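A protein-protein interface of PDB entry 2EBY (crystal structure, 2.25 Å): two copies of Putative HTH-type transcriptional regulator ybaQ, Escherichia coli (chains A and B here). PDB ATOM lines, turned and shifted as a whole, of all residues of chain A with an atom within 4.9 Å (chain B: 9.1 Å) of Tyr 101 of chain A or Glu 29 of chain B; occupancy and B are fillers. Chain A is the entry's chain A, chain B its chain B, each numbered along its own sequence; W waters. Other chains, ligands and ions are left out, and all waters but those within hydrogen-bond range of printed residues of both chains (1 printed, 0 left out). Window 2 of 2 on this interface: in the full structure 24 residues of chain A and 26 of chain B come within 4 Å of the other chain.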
ATOM      1  N   GLU A  96       1.846 -34.913  28.271  1.00  0.00           N
ATOM      2  CA  GLU A  96       1.537 -33.624  27.663  1.00  0.00           C
ATOM      3  C   GLU A  96       2.668 -33.240  26.709  1.00  0.00           C
ATOM      4  O   GLU A  96       3.847 -33.342  27.056  1.00  0.00           O
ATOM      5  CB  GLU A  96       1.385 -32.553  28.750  1.00  0.00           C
ATOM      6  CG  GLU A  96       1.253 -31.129  28.228  1.00  0.00           C
ATOM      7  CD  GLU A  96       1.052 -30.113  29.347  1.00  0.00           C
ATOM      8  OE1 GLU A  96       1.728 -30.219  30.391  1.00  0.00           O
ATOM      9  OE2 GLU A  96       0.226 -29.196  29.180  1.00  0.00           O
ATOM     10  N   THR A  97       2.305 -32.794  25.510  1.00  0.00           N
ATOM     11  CA  THR A  97       3.298 -32.404  24.517  1.00  0.00           C
ATOM     12  C   THR A  97       3.919 -31.057  24.883  1.00  0.00           C
ATOM     13  O   THR A  97       3.374 -30.315  25.699  1.00  0.00           O
ATOM     14  CB  THR A  97       2.670 -32.301  23.119  1.00  0.00           C
ATOM     15  OG1 THR A  97       1.901 -31.096  23.029  1.00  0.00           O
ATOM     16  CG2 THR A  97       1.750 -33.484  22.865  1.00  0.00           C
ATOM     17  N   VAL A  98       5.062 -30.745  24.283  1.00  0.00           N
ATOM     18  CA  VAL A  98       5.742 -29.489  24.560  1.00  0.00           C
ATOM     19  C   VAL A  98       4.983 -28.297  23.972  1.00  0.00           C
ATOM     20  O   VAL A  98       5.062 -27.183  24.487  1.00  0.00           O
ATOM     21  CB  VAL A  98       7.179 -29.511  23.998  1.00  0.00           C
ATOM     22  CG1 VAL A  98       7.166 -29.301  22.493  1.00  0.00           C
ATOM     23  CG2 VAL A  98       8.015 -28.468  24.680  1.00  0.00           C
ATOM     24  N   ALA A  99       4.250 -28.533  22.889  1.00  0.00           N
ATOM     25  CA  ALA A  99       3.465 -27.480  22.250  1.00  0.00           C
ATOM     26  C   ALA A  99       2.365 -27.025  23.203  1.00  0.00           C
ATOM     27  O   ALA A  99       2.106 -25.829  23.352  1.00  0.00           O
ATOM     28  CB  ALA A  99       2.848 -27.994  20.963  1.00  0.00           C
ATOM     29  N   GLU A 100       1.712 -27.999  23.829  1.00  0.00           N
ATOM     30  CA  GLU A 100       0.650 -27.733  24.783  1.00  0.00           C
ATOM     31  C   GLU A 100       1.234 -27.053  26.008  1.00  0.00           C
ATOM     32  O   GLU A 100       0.760 -25.991  26.427  1.00  0.00           O
ATOM     33  CB  GLU A 100      -0.023 -29.037  25.196  1.00  0.00           C
ATOM     34  CG  GLU A 100      -0.929 -29.623  24.137  1.00  0.00           C
ATOM     35  CD  GLU A 100      -1.369 -31.026  24.478  1.00  0.00           C
ATOM     36  OE1 GLU A 100      -2.410 -31.469  23.953  1.00  0.00           O
ATOM     37  OE2 GLU A 100      -0.663 -31.690  25.267  1.00  0.00           O
ATOM     38  N   TYR A 101       2.270 -27.665  26.572  1.00  0.00           N
ATOM     39  CA  TYR A 101       2.918 -27.122  27.759  1.00  0.00           C
ATOM     40  C   TYR A 101       3.355 -25.671  27.589  1.00  0.00           C
ATOM     41  O   TYR A 101       3.080 -24.831  28.444  1.00  0.00           O
ATOM     42  CB  TYR A 101       4.140 -27.954  28.148  1.00  0.00           C
ATOM     43  CG  TYR A 101       4.873 -27.379  29.338  1.00  0.00           C
ATOM     44  CD1 TYR A 101       4.311 -27.429  30.614  1.00  0.00           C
ATOM     45  CD2 TYR A 101       6.087 -26.714  29.179  1.00  0.00           C
ATOM     46  CE1 TYR A 101       4.944 -26.835  31.705  1.00  0.00           C
ATOM     47  CE2 TYR A 101       6.727 -26.118  30.256  1.00  0.00           C
ATOM     48  CZ  TYR A 101       6.147 -26.175  31.516  1.00  0.00           C
ATOM     49  OH  TYR A 101       6.764 -25.573  32.589  1.00  0.00           O
ATOM     50  N   LEU A 102       4.054 -25.377  26.499  1.00  0.00           N
ATOM     51  CA  LEU A 102       4.516 -24.015  26.272  1.00  0.00           C
ATOM     52  C   LEU A 102       3.347 -23.043  26.179  1.00  0.00           C
ATOM     53  O   LEU A 102       3.451 -21.905  26.621  1.00  0.00           O
ATOM     54  CB  LEU A 102       5.361 -23.935  25.000  1.00  0.00           C
ATOM     55  CG  LEU A 102       6.728 -24.610  25.085  1.00  0.00           C
ATOM     56  CD1 LEU A 102       7.479 -24.373  23.789  1.00  0.00           C
ATOM     57  CD2 LEU A 102       7.513 -24.058  26.267  1.00  0.00           C
ATOM     58  N   ALA A 103       2.235 -23.487  25.605  1.00  0.00           N
ATOM     59  CA  ALA A 103       1.069 -22.623  25.494  1.00  0.00           C
ATOM     60  C   ALA A 103       0.618 -22.287  26.909  1.00  0.00           C
ATOM     61  O   ALA A 103       0.467 -21.117  27.261  1.00  0.00           O
ATOM     62  CB  ALA A 103      -0.040 -23.327  24.746  1.00  0.00           C
ATOM     63  N   ARG A 104       0.415 -23.321  27.720  1.00  0.00           N
ATOM     64  CA  ARG A 104      -0.008 -23.131  29.101  1.00  0.00           C
ATOM     65  C   ARG A 104       0.963 -22.256  29.886  1.00  0.00           C
ATOM     66  O   ARG A 104       0.544 -21.354  30.611  1.00  0.00           O
ATOM     67  CB  ARG A 104      -0.174 -24.484  29.795  1.00  0.00           C
ATOM     68  CG  ARG A 104      -1.612 -24.982  29.824  1.00  0.00           C
ATOM     69  CD  ARG A 104      -1.749 -26.456  30.225  1.00  0.00           C
ATOM     70  NE  ARG A 104      -1.083 -26.802  31.478  1.00  0.00           N
ATOM     71  CZ  ARG A 104       0.206 -27.114  31.575  1.00  0.00           C
ATOM     72  NH1 ARG A 104       0.969 -27.122  30.489  1.00  0.00           N
ATOM     73  NH2 ARG A 104       0.732 -27.427  32.751  1.00  0.00           N
ATOM     74  N   ARG A 105       2.258 -22.511  29.731  1.00  0.00           N
ATOM     75  CA  ARG A 105       3.274 -21.739  30.441  1.00  0.00           C
ATOM     76  C   ARG A 105       3.218 -20.242  30.148  1.00  0.00           C
ATOM     77  O   ARG A 105       3.400 -19.423  31.050  1.00  0.00           O
ATOM     78  CB  ARG A 105       4.682 -22.267  30.118  1.00  0.00           C
ATOM     79  CG  ARG A 105       5.784 -21.553  30.899  1.00  0.00           C
ATOM     80  CD  ARG A 105       7.153 -22.192  30.717  1.00  0.00           C
ATOM     81  NE  ARG A 105       7.744 -21.919  29.410  1.00  0.00           N
ATOM     82  CZ  ARG A 105       8.974 -22.290  29.067  1.00  0.00           C
ATOM     83  NH1 ARG A 105       9.734 -22.947  29.936  1.00  0.00           N
ATOM     84  NH2 ARG A 105       9.450 -21.996  27.866  1.00  0.00           N
ATOM     85  N   LEU B  20      15.673 -28.120  24.013  1.00  0.00           N
ATOM     86  CA  LEU B  20      15.709 -27.426  25.293  1.00  0.00           C
ATOM     87  C   LEU B  20      16.177 -25.984  25.226  1.00  0.00           C
ATOM     88  O   LEU B  20      15.496 -25.097  25.734  1.00  0.00           O
ATOM     89  CB  LEU B  20      16.566 -28.191  26.310  1.00  0.00           C
ATOM     90  CG  LEU B  20      16.110 -29.602  26.694  1.00  0.00           C
ATOM     91  CD1 LEU B  20      16.886 -30.080  27.906  1.00  0.00           C
ATOM     92  CD2 LEU B  20      14.634 -29.594  27.004  1.00  0.00           C
ATOM     93  N   LEU B  23      13.873 -23.691  22.903  1.00  0.00           N
ATOM     94  CA  LEU B  23      12.556 -23.488  23.495  1.00  0.00           C
ATOM     95  C   LEU B  23      12.572 -22.909  24.909  1.00  0.00           C
ATOM     96  O   LEU B  23      11.511 -22.697  25.501  1.00  0.00           O
ATOM     97  CB  LEU B  23      11.775 -24.809  23.501  1.00  0.00           C
ATOM     98  CG  LEU B  23      11.551 -25.469  22.136  1.00  0.00           C
ATOM     99  CD1 LEU B  23      10.861 -26.812  22.307  1.00  0.00           C
ATOM    100  CD2 LEU B  23      10.720 -24.542  21.256  1.00  0.00           C
ATOM    101  N   ASP B  24      13.761 -22.655  25.448  1.00  0.00           N
ATOM    102  CA  ASP B  24      13.881 -22.110  26.794  1.00  0.00           C
ATOM    103  C   ASP B  24      13.138 -23.042  27.742  1.00  0.00           C
ATOM    104  O   ASP B  24      12.321 -22.616  28.559  1.00  0.00           O
ATOM    105  CB  ASP B  24      13.285 -20.700  26.842  1.00  0.00           C
ATOM    106  CG  ASP B  24      13.525 -20.009  28.169  1.00  0.00           C
ATOM    107  OD1 ASP B  24      14.632 -20.160  28.727  1.00  0.00           O
ATOM    108  OD2 ASP B  24      12.613 -19.302  28.649  1.00  0.00           O
ATOM    109  N   LEU B  25      13.431 -24.328  27.614  1.00  0.00           N
ATOM    110  CA  LEU B  25      12.797 -25.344  28.431  1.00  0.00           C
ATOM    111  C   LEU B  25      13.824 -25.930  29.400  1.00  0.00           C
ATOM    112  O   LEU B  25      14.941 -26.254  29.003  1.00  0.00           O
ATOM    113  CB  LEU B  25      12.233 -26.438  27.526  1.00  0.00           C
ATOM    114  CG  LEU B  25      11.366 -27.520  28.165  1.00  0.00           C
ATOM    115  CD1 LEU B  25      10.076 -26.899  28.700  1.00  0.00           C
ATOM    116  CD2 LEU B  25      11.057 -28.591  27.137  1.00  0.00           C
ATOM    117  N   LYS B  26      13.456 -26.057  30.669  1.00  0.00           N
ATOM    118  CA  LYS B  26      14.380 -26.614  31.652  1.00  0.00           C
ATOM    119  C   LYS B  26      14.294 -28.129  31.734  1.00  0.00           C
ATOM    120  O   LYS B  26      13.263 -28.720  31.424  1.00  0.00           O
ATOM    121  CB  LYS B  26      14.126 -26.012  33.038  1.00  0.00           C
ATOM    122  CG  LYS B  26      14.510 -24.550  33.138  1.00  0.00           C
ATOM    123  CD  LYS B  26      14.560 -24.081  34.579  1.00  0.00           C
ATOM    124  CE  LYS B  26      15.096 -22.651  34.682  1.00  0.00           C
ATOM    125  NZ  LYS B  26      14.201 -21.657  34.029  1.00  0.00           N
ATOM    126  N   ILE B  27      15.391 -28.746  32.159  1.00  0.00           N
ATOM    127  CA  ILE B  27      15.483 -30.196  32.292  1.00  0.00           C
ATOM    128  C   ILE B  27      14.384 -30.764  33.192  1.00  0.00           C
ATOM    129  O   ILE B  27      13.826 -31.831  32.913  1.00  0.00           O
ATOM    130  CB  ILE B  27      16.887 -30.603  32.837  1.00  0.00           C
ATOM    131  CG1 ILE B  27      17.943 -30.328  31.762  1.00  0.00           C
ATOM    132  CG2 ILE B  27      16.908 -32.078  33.233  1.00  0.00           C
ATOM    133  CD1 ILE B  27      19.360 -30.687  32.145  1.00  0.00           C
ATOM    134  N   ASN B  28      14.067 -30.037  34.257  1.00  0.00           N
ATOM    135  CA  ASN B  28      13.039 -30.468  35.189  1.00  0.00           C
ATOM    136  C   ASN B  28      11.648 -30.397  34.567  1.00  0.00           C
ATOM    137  O   ASN B  28      10.783 -31.220  34.865  1.00  0.00           O
ATOM    138  CB  ASN B  28      13.099 -29.617  36.455  1.00  0.00           C
ATOM    139  CG  ASN B  28      13.260 -30.455  37.698  1.00  0.00           C
ATOM    140  OD1 ASN B  28      12.337 -31.162  38.102  1.00  0.00           O
ATOM    141  ND2 ASN B  28      14.442 -30.397  38.306  1.00  0.00           N
ATOM    142  N   GLU B  29      11.436 -29.409  33.705  1.00  0.00           N
ATOM    143  CA  GLU B  29      10.150 -29.272  33.033  1.00  0.00           C
ATOM    144  C   GLU B  29       9.975 -30.438  32.069  1.00  0.00           C
ATOM    145  O   GLU B  29       8.903 -31.031  31.981  1.00  0.00           O
ATOM    146  CB  GLU B  29      10.087 -27.962  32.257  1.00  0.00           C
ATOM    147  CG  GLU B  29      10.136 -26.727  33.125  1.00  0.00           C
ATOM    148  CD  GLU B  29      10.074 -25.462  32.305  1.00  0.00           C
ATOM    149  OE1 GLU B  29      11.047 -25.178  31.572  1.00  0.00           O
ATOM    150  OE2 GLU B  29       9.047 -24.759  32.386  1.00  0.00           O
ATOM    151  N   LEU B  30      11.040 -30.763  31.346  1.00  0.00           N
ATOM    152  CA  LEU B  30      11.002 -31.865  30.402  1.00  0.00           C
ATOM    153  C   LEU B  30      10.718 -33.174  31.129  1.00  0.00           C
ATOM    154  O   LEU B  30       9.903 -33.976  30.677  1.00  0.00           O
ATOM    155  CB  LEU B  30      12.330 -31.969  29.647  1.00  0.00           C
ATOM    156  CG  LEU B  30      12.436 -33.164  28.690  1.00  0.00           C
ATOM    157  CD1 LEU B  30      11.330 -33.099  27.628  1.00  0.00           C
ATOM    158  CD2 LEU B  30      13.792 -33.157  28.029  1.00  0.00           C
ATOM    159  N   ALA B  31      11.396 -33.391  32.257  1.00  0.00           N
ATOM    160  CA  ALA B  31      11.196 -34.612  33.035  1.00  0.00           C
ATOM    161  C   ALA B  31       9.728 -34.743  33.428  1.00  0.00           C
ATOM    162  O   ALA B  31       9.178 -35.830  33.406  1.00  0.00           O
ATOM    163  CB  ALA B  31      12.081 -34.611  34.285  1.00  0.00           C
ATOM    164  N   GLU B  32       9.102 -33.628  33.786  1.00  0.00           N
ATOM    165  CA  GLU B  32       7.693 -33.633  34.162  1.00  0.00           C
ATOM    166  C   GLU B  32       6.843 -33.982  32.947  1.00  0.00           C
ATOM    167  O   GLU B  32       5.921 -34.796  33.031  1.00  0.00           O
ATOM    168  CB  GLU B  32       7.287 -32.259  34.691  1.00  0.00           C
ATOM    169  CG  GLU B  32       7.017 -32.208  36.179  1.00  0.00           C
ATOM    170  CD  GLU B  32       6.741 -30.798  36.664  1.00  0.00           C
ATOM    171  OE1 GLU B  32       7.511 -30.319  37.522  1.00  0.00           O
ATOM    172  OE2 GLU B  32       5.768 -30.168  36.188  1.00  0.00           O
ATOM    173  N   LEU B  33       7.145 -33.346  31.817  1.00  0.00           N
ATOM    174  CA  LEU B  33       6.415 -33.624  30.588  1.00  0.00           C
ATOM    175  C   LEU B  33       6.557 -35.108  30.241  1.00  0.00           C
ATOM    176  O   LEU B  33       5.581 -35.755  29.861  1.00  0.00           O
ATOM    177  CB  LEU B  33       6.961 -32.782  29.428  1.00  0.00           C
ATOM    178  CG  LEU B  33       6.792 -31.261  29.476  1.00  0.00           C
ATOM    179  CD1 LEU B  33       7.310 -30.652  28.195  1.00  0.00           C
ATOM    180  CD2 LEU B  33       5.327 -30.907  29.653  1.00  0.00           C
ATOM    181  N   LEU B  34       7.773 -35.637  30.385  1.00  0.00           N
ATOM    182  CA  LEU B  34       8.060 -37.036  30.073  1.00  0.00           C
ATOM    183  C   LEU B  34       7.533 -38.028  31.108  1.00  0.00           C
ATOM    184  O   LEU B  34       7.270 -39.181  30.784  1.00  0.00           O
ATOM    185  CB  LEU B  34       9.570 -37.242  29.911  1.00  0.00           C
ATOM    186  CG  LEU B  34      10.273 -36.578  28.718  1.00  0.00           C
ATOM    187  CD1 LEU B  34      11.764 -36.632  28.928  1.00  0.00           C
ATOM    188  CD2 LEU B  34       9.894 -37.284  27.414  1.00  0.00           C
ATOM    189  N   HIS B  35       7.373 -37.572  32.344  1.00  0.00           N
ATOM    190  CA  HIS B  35       6.900 -38.415  33.439  1.00  0.00           C
ATOM    191  C   HIS B  35       7.980 -39.410  33.846  1.00  0.00           C
ATOM    192  O   HIS B  35       7.727 -40.610  33.961  1.00  0.00           O
ATOM    193  CB  HIS B  35       5.625 -39.173  33.057  1.00  0.00           C
ATOM    194  CG  HIS B  35       4.957 -39.851  34.215  1.00  0.00           C
ATOM    195  ND1 HIS B  35       4.302 -39.152  35.206  1.00  0.00           N
ATOM    196  CD2 HIS B  35       4.874 -41.158  34.558  1.00  0.00           C
ATOM    197  CE1 HIS B  35       3.843 -40.003  36.112  1.00  0.00           C
ATOM    198  NE2 HIS B  35       4.178 -41.225  35.740  1.00  0.00           N
ATOM    199  N   VAL B  36       9.187 -38.889  34.042  1.00  0.00           N
ATOM    200  CA  VAL B  36      10.337 -39.680  34.471  1.00  0.00           C
ATOM    201  C   VAL B  36      11.092 -38.847  35.498  1.00  0.00           C
ATOM    202  O   VAL B  36      10.795 -37.672  35.690  1.00  0.00           O
ATOM    203  CB  VAL B  36      11.325 -40.017  33.297  1.00  0.00           C
ATOM    204  CG1 VAL B  36      10.605 -40.767  32.194  1.00  0.00           C
ATOM    205  CG2 VAL B  36      11.964 -38.744  32.758  1.00  0.00           C
ATOM    206  N   ARG B  38      14.145 -36.657  37.047  1.00  0.00           N
ATOM    207  CA  ARG B  38      15.059 -35.683  36.459  1.00  0.00           C
ATOM    208  C   ARG B  38      16.375 -36.364  36.093  1.00  0.00           C
ATOM    209  O   ARG B  38      16.952 -36.105  35.036  1.00  0.00           O
ATOM    210  CB  ARG B  38      15.353 -34.547  37.446  1.00  0.00           C
ATOM    211  CG  ARG B  38      16.247 -33.437  36.870  1.00  0.00           C
ATOM    212  CD  ARG B  38      17.312 -32.933  37.859  1.00  0.00           C
ATOM    213  NE  ARG B  38      17.767 -31.584  37.512  1.00  0.00           N
ATOM    214  CZ  ARG B  38      18.878 -31.009  37.975  1.00  0.00           C
ATOM    215  NH1 ARG B  38      19.673 -31.660  38.811  1.00  0.00           N
ATOM    216  NH2 ARG B  38      19.190 -29.774  37.603  1.00  0.00           N
ATOM    217  N   VAL B  41      16.631 -37.766  32.598  1.00  0.00           N
ATOM    218  CA  VAL B  41      16.824 -36.815  31.513  1.00  0.00           C
ATOM    219  C   VAL B  41      18.285 -36.375  31.478  1.00  0.00           C
ATOM    220  O   VAL B  41      18.920 -36.408  30.425  1.00  0.00           O
ATOM    221  CB  VAL B  41      15.930 -35.572  31.662  1.00  0.00           C
ATOM    222  CG1 VAL B  41      16.220 -34.597  30.533  1.00  0.00           C
ATOM    223  CG2 VAL B  41      14.453 -35.973  31.619  1.00  0.00           C
ATOM    224  N   VAL B  62       6.247 -36.093  23.450  1.00  0.00           N
ATOM    225  CA  VAL B  62       6.459 -34.718  23.854  1.00  0.00           C
ATOM    226  C   VAL B  62       6.777 -33.780  22.700  1.00  0.00           C
ATOM    227  O   VAL B  62       6.167 -32.716  22.568  1.00  0.00           O
ATOM    228  CB  VAL B  62       7.596 -34.620  24.892  1.00  0.00           C
ATOM    229  CG1 VAL B  62       8.001 -33.171  25.101  1.00  0.00           C
ATOM    230  CG2 VAL B  62       7.140 -35.223  26.210  1.00  0.00           C
ATOM    231  N   PHE B  63       7.721 -34.191  21.857  1.00  0.00           N
ATOM    232  CA  PHE B  63       8.173 -33.365  20.753  1.00  0.00           C
ATOM    233  C   PHE B  63       7.512 -33.592  19.399  1.00  0.00           C
ATOM    234  O   PHE B  63       7.875 -32.935  18.426  1.00  0.00           O
ATOM    235  CB  PHE B  63       9.692 -33.497  20.632  1.00  0.00           C
ATOM    236  CG  PHE B  63      10.427 -33.002  21.845  1.00  0.00           C
ATOM    237  CD1 PHE B  63      10.409 -31.645  22.180  1.00  0.00           C
ATOM    238  CD2 PHE B  63      11.090 -33.888  22.682  1.00  0.00           C
ATOM    239  CE1 PHE B  63      11.033 -31.182  23.329  1.00  0.00           C
ATOM    240  CE2 PHE B  63      11.721 -33.439  23.837  1.00  0.00           C
ATOM    241  CZ  PHE B  63      11.692 -32.087  24.164  1.00  0.00           C
HETATM  242  O   HOH W   1       4.853 -30.943  20.972  1.00  0.00           O
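The backbone carbonyl oxygen (O) of Val 62 of chain B lies within hydrogen-bond range of the backbone NH (N) of Val 98 of chain A, at 2.8 Å. The side-chain carboxylate of Glu 29 of chain B lies within salt-bridge range of the guanidinium group of Arg 105 of chain A (3.1 Å). The guanidinium group of Arg 105 of chain A is in hydrogen-bond range of the backbone carbonyl oxygen of Asp 24 of chain B (2.9 Å). The side-chain carboxylate (OE2) of Glu 29 of chain B lies within hydrogen-bond range of the side-chain hydroxyl (OH) of Tyr 101 of chain A. NH2 of Arg 105 of chain A sits at hydrogen-bond distance from O of Leu 23 of chain B.
NH1 of Arg 104 of chain A lies within salt-bridge range of OE2 of Glu 96 of chain A, 2.6 Å away. The backbone carbonyl oxygen (O) of Leu 20 of chain B lies within hydrogen-bond range of the backbone NH (N) of Leu 25 of chain B (2.9 Å). The backbone NH (N) of Thr 97 of chain A is in hydrogen-bond range of the side-chain carboxylate (OE2) of Glu 100 of chain A (3.2 Å). OE1 of Glu 29 of chain B lies within hydrogen-bond range of N of Lys 26 of chain B, at 2.7 Å. The backbone NH (N) of Ala 99 of chain A sits close to the side-chain hydroxyl (OG1) of Thr 97 of chain A, at 3.5 Å.
Among the printed residues, pairs that only touch across the chains: Glu 96 of chain A with Leu 33 of chain B (3.7 Å), Glu 96 of chain A with Val 62 of chain B (3.9 Å), Thr 97 of chain A with Val 62 of chain B (3.5 Å), Val 98 of chain A with Leu 25 of chain B (3.9 Å), Tyr 101 of chain A with Leu 25 of chain B (3.8 Å) and Tyr 101 of chain A with Leu 33 of chain B (3.5 Å).
Printed residues of chain B within 4 Å of Tyr 101 of chain A: Leu 25 (3.8 Å), Glu 29 (2.4 Å) and Leu 33 (3.5 Å). Printed residues of chain B within 4 Å of Val 98 of chain A: Leu 25 and Val 62. Printed residues of chain B within 4 Å of Thr 97 of chain A: Val 62. Printed residues of chain A within 4 Å of Leu 25 of chain B: Val 98 (3.9 Å) and Tyr 101 (3.8 Å). Asn 28 of chain B touches none of the printed residues of chain A. The nearest printed residue of chain A that does not touch Glu 29 of chain B is Leu 102 of chain A (6.3 Å). The nearest printed residue of chain B that does not touch Thr 97 of chain A is Leu 33 of chain B (4.4 Å).
Of the 10 printed residues of chain A, 5 touch a printed residue of chain B. Printed residues of chain A that touch a printed residue of chain B: Glu 96, Thr 97, Val 98, Tyr 101 and Arg 105. Among the printed residues, Asp or Glu carboxylates within 4 Å of a Lys or Arg side-chain nitrogen of the other chain: Arg 105 of chain A with Glu 29 of chain B.
No position is printed for both chains. Of the 11 pairs that touch across the chains among the printed residues, none has its exchanged pair printed and touching as well.
Water W1 lies within hydrogen-bond range of O of Val 62 of chain B (2.7 Å), N of Ala 99 of chain A (3.1 Å) and N of Val 98 of chain A (3.3 Å).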
